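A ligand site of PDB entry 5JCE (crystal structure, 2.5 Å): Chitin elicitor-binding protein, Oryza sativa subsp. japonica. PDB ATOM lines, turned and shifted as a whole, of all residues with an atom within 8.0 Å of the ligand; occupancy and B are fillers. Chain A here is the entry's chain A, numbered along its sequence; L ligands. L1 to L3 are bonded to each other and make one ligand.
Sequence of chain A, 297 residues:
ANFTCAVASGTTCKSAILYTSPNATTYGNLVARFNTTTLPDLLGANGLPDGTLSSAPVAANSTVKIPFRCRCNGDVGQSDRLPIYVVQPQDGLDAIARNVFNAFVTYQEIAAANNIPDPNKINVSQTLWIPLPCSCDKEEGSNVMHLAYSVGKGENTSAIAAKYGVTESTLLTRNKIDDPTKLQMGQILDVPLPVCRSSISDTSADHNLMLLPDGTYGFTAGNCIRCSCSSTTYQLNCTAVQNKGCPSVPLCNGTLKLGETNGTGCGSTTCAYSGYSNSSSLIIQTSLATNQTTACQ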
ATOM      1  N   ARG A  81     -27.582 -10.456 -26.717  1.00  0.00           N
ATOM      2  CA  ARG A  81     -28.090 -11.806 -26.412  1.00  0.00           C
ATOM      3  C   ARG A  81     -28.495 -12.611 -27.645  1.00  0.00           C
ATOM      4  O   ARG A  81     -29.131 -13.670 -27.538  1.00  0.00           O
ATOM      5  CB  ARG A  81     -29.294 -11.720 -25.478  1.00  0.00           C
ATOM      6  CG  ARG A  81     -29.188 -10.633 -24.417  1.00  0.00           C
ATOM      7  CD  ARG A  81     -27.933 -10.748 -23.582  1.00  0.00           C
ATOM      8  NE  ARG A  81     -27.962  -9.723 -22.543  1.00  0.00           N
ATOM      9  CZ  ARG A  81     -28.989  -9.503 -21.738  1.00  0.00           C
ATOM     10  NH1 ARG A  81     -30.070 -10.274 -21.794  1.00  0.00           N
ATOM     11  NH2 ARG A  81     -28.937  -8.523 -20.838  1.00  0.00           N
ATOM     12  N   LEU A  82     -28.153 -12.083 -28.809  1.00  0.00           N
ATOM     13  CA  LEU A  82     -28.245 -12.816 -30.058  1.00  0.00           C
ATOM     14  C   LEU A  82     -26.847 -12.677 -30.651  1.00  0.00           C
ATOM     15  O   LEU A  82     -26.135 -11.738 -30.293  1.00  0.00           O
ATOM     16  CB  LEU A  82     -29.334 -12.238 -30.960  1.00  0.00           C
ATOM     17  CG  LEU A  82     -30.757 -12.251 -30.398  1.00  0.00           C
ATOM     18  CD1 LEU A  82     -31.661 -11.448 -31.291  1.00  0.00           C
ATOM     19  CD2 LEU A  82     -31.268 -13.671 -30.292  1.00  0.00           C
ATOM     20  N   PRO A  83     -26.441 -13.617 -31.520  1.00  0.00           N
ATOM     21  CA  PRO A  83     -27.201 -14.802 -31.886  1.00  0.00           C
ATOM     22  C   PRO A  83     -27.110 -15.913 -30.843  1.00  0.00           C
ATOM     23  O   PRO A  83     -26.303 -15.890 -29.908  1.00  0.00           O
ATOM     24  CB  PRO A  83     -26.544 -15.243 -33.185  1.00  0.00           C
ATOM     25  CG  PRO A  83     -25.153 -14.822 -33.047  1.00  0.00           C
ATOM     26  CD  PRO A  83     -25.175 -13.533 -32.275  1.00  0.00           C
ATOM     27  N   ILE A  84     -27.971 -16.907 -31.030  1.00  0.00           N
ATOM     28  CA  ILE A  84     -28.019 -18.056 -30.169  1.00  0.00           C
ATOM     29  C   ILE A  84     -27.652 -19.288 -30.954  1.00  0.00           C
ATOM     30  O   ILE A  84     -28.331 -19.663 -31.912  1.00  0.00           O
ATOM     31  CB  ILE A  84     -29.408 -18.241 -29.541  1.00  0.00           C
ATOM     32  CG1 ILE A  84     -29.634 -17.144 -28.495  1.00  0.00           C
ATOM     33  CG2 ILE A  84     -29.498 -19.600 -28.882  1.00  0.00           C
ATOM     34  CD1 ILE A  84     -31.062 -17.085 -27.930  1.00  0.00           C
ATOM     35  N   TYR A  85     -26.567 -19.932 -30.536  1.00  0.00           N
ATOM     36  CA  TYR A  85     -26.097 -21.133 -31.195  1.00  0.00           C
ATOM     37  C   TYR A  85     -26.485 -22.380 -30.396  1.00  0.00           C
ATOM     38  O   TYR A  85     -26.342 -22.416 -29.180  1.00  0.00           O
ATOM     39  CB  TYR A  85     -24.582 -21.053 -31.376  1.00  0.00           C
ATOM     40  CG  TYR A  85     -24.040 -22.224 -32.146  1.00  0.00           C
ATOM     41  CD1 TYR A  85     -24.088 -22.246 -33.525  1.00  0.00           C
ATOM     42  CD2 TYR A  85     -23.488 -23.313 -31.481  1.00  0.00           C
ATOM     43  CE1 TYR A  85     -23.611 -23.321 -34.228  1.00  0.00           C
ATOM     44  CE2 TYR A  85     -22.999 -24.382 -32.184  1.00  0.00           C
ATOM     45  CZ  TYR A  85     -23.062 -24.376 -33.553  1.00  0.00           C
ATOM     46  OH  TYR A  85     -22.587 -25.449 -34.274  1.00  0.00           O
ATOM     47  N   VAL A  86     -27.008 -23.390 -31.092  1.00  0.00           N
ATOM     48  CA  VAL A  86     -27.332 -24.681 -30.500  1.00  0.00           C
ATOM     49  C   VAL A  86     -26.241 -25.713 -30.814  1.00  0.00           C
ATOM     50  O   VAL A  86     -25.997 -26.036 -31.976  1.00  0.00           O
ATOM     51  CB  VAL A  86     -28.675 -25.239 -31.012  1.00  0.00           C
ATOM     52  CG1 VAL A  86     -29.056 -26.499 -30.226  1.00  0.00           C
ATOM     53  CG2 VAL A  86     -29.766 -24.190 -30.905  1.00  0.00           C
ATOM     54  N   ILE A 110     -16.978 -16.540 -25.454  1.00  0.00           N
ATOM     55  CA  ILE A 110     -18.197 -17.336 -25.481  1.00  0.00           C
ATOM     56  C   ILE A 110     -18.486 -17.906 -24.087  1.00  0.00           C
ATOM     57  O   ILE A 110     -19.571 -17.696 -23.553  1.00  0.00           O
ATOM     58  CB  ILE A 110     -18.118 -18.504 -26.475  1.00  0.00           C
ATOM     59  CG1 ILE A 110     -17.829 -18.010 -27.884  1.00  0.00           C
ATOM     60  CG2 ILE A 110     -19.422 -19.308 -26.464  1.00  0.00           C
ATOM     61  CD1 ILE A 110     -17.927 -19.101 -28.923  1.00  0.00           C
ATOM     62  N   ALA A 111     -17.521 -18.625 -23.525  1.00  0.00           N
ATOM     63  CA  ALA A 111     -17.670 -19.264 -22.216  1.00  0.00           C
ATOM     64  C   ALA A 111     -17.999 -18.229 -21.148  1.00  0.00           C
ATOM     65  O   ALA A 111     -18.912 -18.425 -20.356  1.00  0.00           O
ATOM     66  CB  ALA A 111     -16.412 -20.026 -21.833  1.00  0.00           C
ATOM     67  N   ALA A 112     -17.273 -17.129 -21.145  1.00  0.00           N
ATOM     68  CA  ALA A 112     -17.568 -16.067 -20.203  1.00  0.00           C
ATOM     69  C   ALA A 112     -18.995 -15.549 -20.377  1.00  0.00           C
ATOM     70  O   ALA A 112     -19.655 -15.208 -19.399  1.00  0.00           O
ATOM     71  CB  ALA A 112     -16.563 -14.937 -20.341  1.00  0.00           C
ATOM     72  N   ALA A 113     -19.482 -15.510 -21.608  1.00  0.00           N
ATOM     73  CA  ALA A 113     -20.816 -14.972 -21.873  1.00  0.00           C
ATOM     74  C   ALA A 113     -21.928 -15.915 -21.394  1.00  0.00           C
ATOM     75  O   ALA A 113     -23.028 -15.461 -21.058  1.00  0.00           O
ATOM     76  CB  ALA A 113     -20.985 -14.656 -23.358  1.00  0.00           C
ATOM     77  N   ASN A 114     -21.632 -17.215 -21.350  1.00  0.00           N
ATOM     78  CA  ASN A 114     -22.601 -18.249 -20.947  1.00  0.00           C
ATOM     79  C   ASN A 114     -22.262 -18.920 -19.611  1.00  0.00           C
ATOM     80  O   ASN A 114     -22.733 -20.020 -19.321  1.00  0.00           O
ATOM     81  CB  ASN A 114     -22.717 -19.318 -22.047  1.00  0.00           C
ATOM     82  CG  ASN A 114     -23.113 -18.735 -23.401  1.00  0.00           C
ATOM     83  OD1 ASN A 114     -24.294 -18.673 -23.734  1.00  0.00           O
ATOM     84  ND2 ASN A 114     -22.117 -18.317 -24.172  1.00  0.00           N
ATOM     85  N   ASN A 115     -21.458 -18.235 -18.799  1.00  0.00           N
ATOM     86  CA  ASN A 115     -21.047 -18.692 -17.483  1.00  0.00           C
ATOM     87  C   ASN A 115     -20.481 -20.112 -17.439  1.00  0.00           C
ATOM     88  O   ASN A 115     -20.593 -20.804 -16.429  1.00  0.00           O
ATOM     89  CB  ASN A 115     -22.212 -18.591 -16.515  1.00  0.00           C
ATOM     90  CG  ASN A 115     -21.772 -18.206 -15.111  1.00  0.00           C
ATOM     91  OD1 ASN A 115     -20.619 -18.413 -14.740  1.00  0.00           O
ATOM     92  ND2 ASN A 115     -22.701 -17.653 -14.326  1.00  0.00           N
ATOM     93  N   ILE A 116     -19.886 -20.557 -18.542  1.00  0.00           N
ATOM     94  CA  ILE A 116     -19.312 -21.900 -18.612  1.00  0.00           C
ATOM     95  C   ILE A 116     -17.922 -21.906 -17.976  1.00  0.00           C
ATOM     96  O   ILE A 116     -17.039 -21.166 -18.389  1.00  0.00           O
ATOM     97  CB  ILE A 116     -19.252 -22.387 -20.080  1.00  0.00           C
ATOM     98  CG1 ILE A 116     -20.679 -22.569 -20.613  1.00  0.00           C
ATOM     99  CG2 ILE A 116     -18.470 -23.668 -20.207  1.00  0.00           C
ATOM    100  CD1 ILE A 116     -20.769 -22.603 -22.119  1.00  0.00           C
ATOM    101  N   SER A 125     -27.118 -29.839 -27.767  1.00  0.00           N
ATOM    102  CA  SER A 125     -28.396 -29.136 -27.614  1.00  0.00           C
ATOM    103  C   SER A 125     -28.331 -27.968 -26.623  1.00  0.00           C
ATOM    104  O   SER A 125     -29.338 -27.278 -26.394  1.00  0.00           O
ATOM    105  CB  SER A 125     -29.516 -30.093 -27.200  1.00  0.00           C
ATOM    106  OG  SER A 125     -29.559 -31.228 -28.049  1.00  0.00           O
ATOM    107  N   GLN A 126     -27.161 -27.722 -26.044  1.00  0.00           N
ATOM    108  CA  GLN A 126     -26.977 -26.583 -25.156  1.00  0.00           C
ATOM    109  C   GLN A 126     -26.997 -25.287 -25.973  1.00  0.00           C
ATOM    110  O   GLN A 126     -26.452 -25.225 -27.073  1.00  0.00           O
ATOM    111  CB  GLN A 126     -25.683 -26.697 -24.346  1.00  0.00           C
ATOM    112  CG  GLN A 126     -25.484 -25.603 -23.318  1.00  0.00           C
ATOM    113  CD  GLN A 126     -24.111 -25.655 -22.646  1.00  0.00           C
ATOM    114  OE1 GLN A 126     -23.371 -26.641 -22.783  1.00  0.00           O
ATOM    115  NE2 GLN A 126     -23.749 -24.579 -21.961  1.00  0.00           N
ATOM    116  N   THR A 127     -27.630 -24.247 -25.463  1.00  0.00           N
ATOM    117  CA  THR A 127     -27.678 -23.022 -26.211  1.00  0.00           C
ATOM    118  C   THR A 127     -26.678 -22.037 -25.677  1.00  0.00           C
ATOM    119  O   THR A 127     -26.445 -21.941 -24.469  1.00  0.00           O
ATOM    120  CB  THR A 127     -29.071 -22.387 -26.228  1.00  0.00           C
ATOM    121  OG1 THR A 127     -29.485 -22.091 -24.890  1.00  0.00           O
ATOM    122  CG2 THR A 127     -30.061 -23.328 -26.902  1.00  0.00           C
ATOM    123  N   LEU A 128     -26.094 -21.303 -26.622  1.00  0.00           N
ATOM    124  CA  LEU A 128     -24.984 -20.404 -26.378  1.00  0.00           C
ATOM    125  C   LEU A 128     -25.296 -19.057 -26.963  1.00  0.00           C
ATOM    126  O   LEU A 128     -25.560 -18.926 -28.156  1.00  0.00           O
ATOM    127  CB  LEU A 128     -23.710 -20.931 -27.029  1.00  0.00           C
ATOM    128  CG  LEU A 128     -23.117 -22.250 -26.550  1.00  0.00           C
ATOM    129  CD1 LEU A 128     -22.013 -22.678 -27.500  1.00  0.00           C
ATOM    130  CD2 LEU A 128     -22.602 -22.069 -25.132  1.00  0.00           C
ATOM    131  N   TRP A 129     -25.275 -18.048 -26.122  1.00  0.00           N
ATOM    132  CA  TRP A 129     -25.239 -16.710 -26.640  1.00  0.00           C
ATOM    133  C   TRP A 129     -23.843 -16.447 -27.265  1.00  0.00           C
ATOM    134  O   TRP A 129     -22.821 -16.772 -26.685  1.00  0.00           O
ATOM    135  CB  TRP A 129     -25.592 -15.736 -25.525  1.00  0.00           C
ATOM    136  CG  TRP A 129     -25.226 -14.342 -25.782  1.00  0.00           C
ATOM    137  CD1 TRP A 129     -25.301 -13.658 -26.968  1.00  0.00           C
ATOM    138  CD2 TRP A 129     -24.723 -13.418 -24.820  1.00  0.00           C
ATOM    139  NE1 TRP A 129     -24.869 -12.364 -26.798  1.00  0.00           N
ATOM    140  CE2 TRP A 129     -24.512 -12.185 -25.489  1.00  0.00           C
ATOM    141  CE3 TRP A 129     -24.430 -13.513 -23.457  1.00  0.00           C
ATOM    142  CZ2 TRP A 129     -24.019 -11.055 -24.834  1.00  0.00           C
ATOM    143  CZ3 TRP A 129     -23.934 -12.390 -22.809  1.00  0.00           C
ATOM    144  CH2 TRP A 129     -23.725 -11.183 -23.498  1.00  0.00           C
ATOM    145  N   ILE A 130     -23.793 -15.908 -28.469  1.00  0.00           N
ATOM    146  CA  ILE A 130     -22.510 -15.642 -29.082  1.00  0.00           C
ATOM    147  C   ILE A 130     -22.405 -14.164 -29.094  1.00  0.00           C
ATOM    148  O   ILE A 130     -23.157 -13.546 -29.789  1.00  0.00           O
ATOM    149  CB  ILE A 130     -22.507 -16.113 -30.533  1.00  0.00           C
ATOM    150  CG1 ILE A 130     -22.741 -17.619 -30.605  1.00  0.00           C
ATOM    151  CG2 ILE A 130     -21.217 -15.754 -31.217  1.00  0.00           C
ATOM    152  CD1 ILE A 130     -21.862 -18.421 -29.710  1.00  0.00           C
HETATM  153  C1  LIG L   1     -39.567 -22.322 -20.329  1.00  0.00           C
HETATM  154  C2  LIG L   1     -38.558 -21.968 -19.257  1.00  0.00           C
HETATM  155  C3  LIG L   1     -37.352 -21.342 -19.929  1.00  0.00           C
HETATM  156  C4  LIG L   1     -36.828 -22.183 -21.085  1.00  0.00           C
HETATM  157  C5  LIG L   1     -37.957 -22.691 -21.952  1.00  0.00           C
HETATM  158  C6  LIG L   1     -37.443 -23.807 -22.819  1.00  0.00           C
HETATM  159  C7  LIG L   1     -39.236 -21.387 -16.981  1.00  0.00           C
HETATM  160  C8  LIG L   1     -39.564 -20.277 -16.073  1.00  0.00           C
HETATM  161  N1  LIG L   1     -39.165 -21.103 -18.268  1.00  0.00           N
HETATM  162  O1  LIG L   1     -40.693 -22.934 -19.747  1.00  0.00           O
HETATM  163  O2  LIG L   1     -36.310 -21.265 -19.001  1.00  0.00           O
HETATM  164  O3  LIG L   1     -35.927 -21.429 -21.888  1.00  0.00           O
HETATM  165  O4  LIG L   1     -38.971 -23.274 -21.164  1.00  0.00           O
HETATM  166  O5  LIG L   1     -38.049 -24.969 -22.301  1.00  0.00           O
HETATM  167  O6  LIG L   1     -39.041 -22.465 -16.522  1.00  0.00           O
HETATM  168  C1  LG2 L   2     -34.625 -22.043 -21.892  1.00  0.00           C
HETATM  169  C2  LG2 L   2     -33.986 -21.870 -23.259  1.00  0.00           C
HETATM  170  C3  LG2 L   2     -32.499 -22.119 -23.226  1.00  0.00           C
HETATM  171  C4  LG2 L   2     -31.849 -21.416 -22.065  1.00  0.00           C
HETATM  172  C5  LG2 L   2     -32.530 -21.846 -20.813  1.00  0.00           C
HETATM  173  C6  LG2 L   2     -32.032 -21.034 -19.672  1.00  0.00           C
HETATM  174  C7  LG2 L   2     -35.394 -22.217 -25.192  1.00  0.00           C
HETATM  175  C8  LG2 L   2     -35.843 -23.138 -26.261  1.00  0.00           C
HETATM  176  N1  LG2 L   2     -34.583 -22.720 -24.265  1.00  0.00           N
HETATM  177  O1  LG2 L   2     -31.971 -21.582 -24.423  1.00  0.00           O
HETATM  178  O2  LG2 L   2     -30.474 -21.741 -21.942  1.00  0.00           O
HETATM  179  O3  LG2 L   2     -33.833 -21.382 -20.930  1.00  0.00           O
HETATM  180  O4  LG2 L   2     -33.060 -20.076 -19.550  1.00  0.00           O
HETATM  181  O5  LG2 L   2     -35.774 -21.079 -25.151  1.00  0.00           O
HETATM  182  C1  LG3 L   3     -29.685 -20.583 -21.668  1.00  0.00           C
HETATM  183  C2  LG3 L   3     -28.403 -21.053 -21.038  1.00  0.00           C
HETATM  184  C3  LG3 L   3     -27.458 -19.900 -20.901  1.00  0.00           C
HETATM  185  C4  LG3 L   3     -27.181 -19.339 -22.279  1.00  0.00           C
HETATM  186  C5  LG3 L   3     -28.494 -18.823 -22.791  1.00  0.00           C
HETATM  187  C6  LG3 L   3     -28.335 -18.296 -24.195  1.00  0.00           C
HETATM  188  C7  LG3 L   3     -29.044 -22.872 -19.667  1.00  0.00           C
HETATM  189  C8  LG3 L   3     -29.509 -23.319 -18.347  1.00  0.00           C
HETATM  190  N1  LG3 L   3     -28.749 -21.606 -19.778  1.00  0.00           N
HETATM  191  O1  LG3 L   3     -26.268 -20.365 -20.353  1.00  0.00           O
HETATM  192  O2  LG3 L   3     -26.272 -18.255 -22.212  1.00  0.00           O
HETATM  193  O3  LG3 L   3     -29.363 -19.908 -22.866  1.00  0.00           O
HETATM  194  O4  LG3 L   3     -29.603 -18.355 -24.811  1.00  0.00           O
HETATM  195  O5  LG3 L   3     -28.940 -23.647 -20.553  1.00  0.00           O
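Ile 84 touches the ligand. Trp 129 touches the ligand. Hydrophobic or aromatic side chains within 4 Å of the ligand: Ile 84 and Trp 129. Of the 19 residues printed, 4 come within 4 Å of the ligand.
ND2 of Asn 114 lies within hydrogen-bond range of O of Ile 110, at 2.7 Å. The side-chain amide oxygen (OD1) of Asn 114 sits at hydrogen-bond distance from the backbone NH (N) of Trp 129, 2.7 Å away.
The side-chain amide oxygen (OD1) of Asn 114 is in hydrogen-bond range of an oxygen (O2) of LG3 L3, at 2.5 Å. O1 of LG2 L2 sits at hydrogen-bond distance from OG1 of Thr 127, 2.6 Å away.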
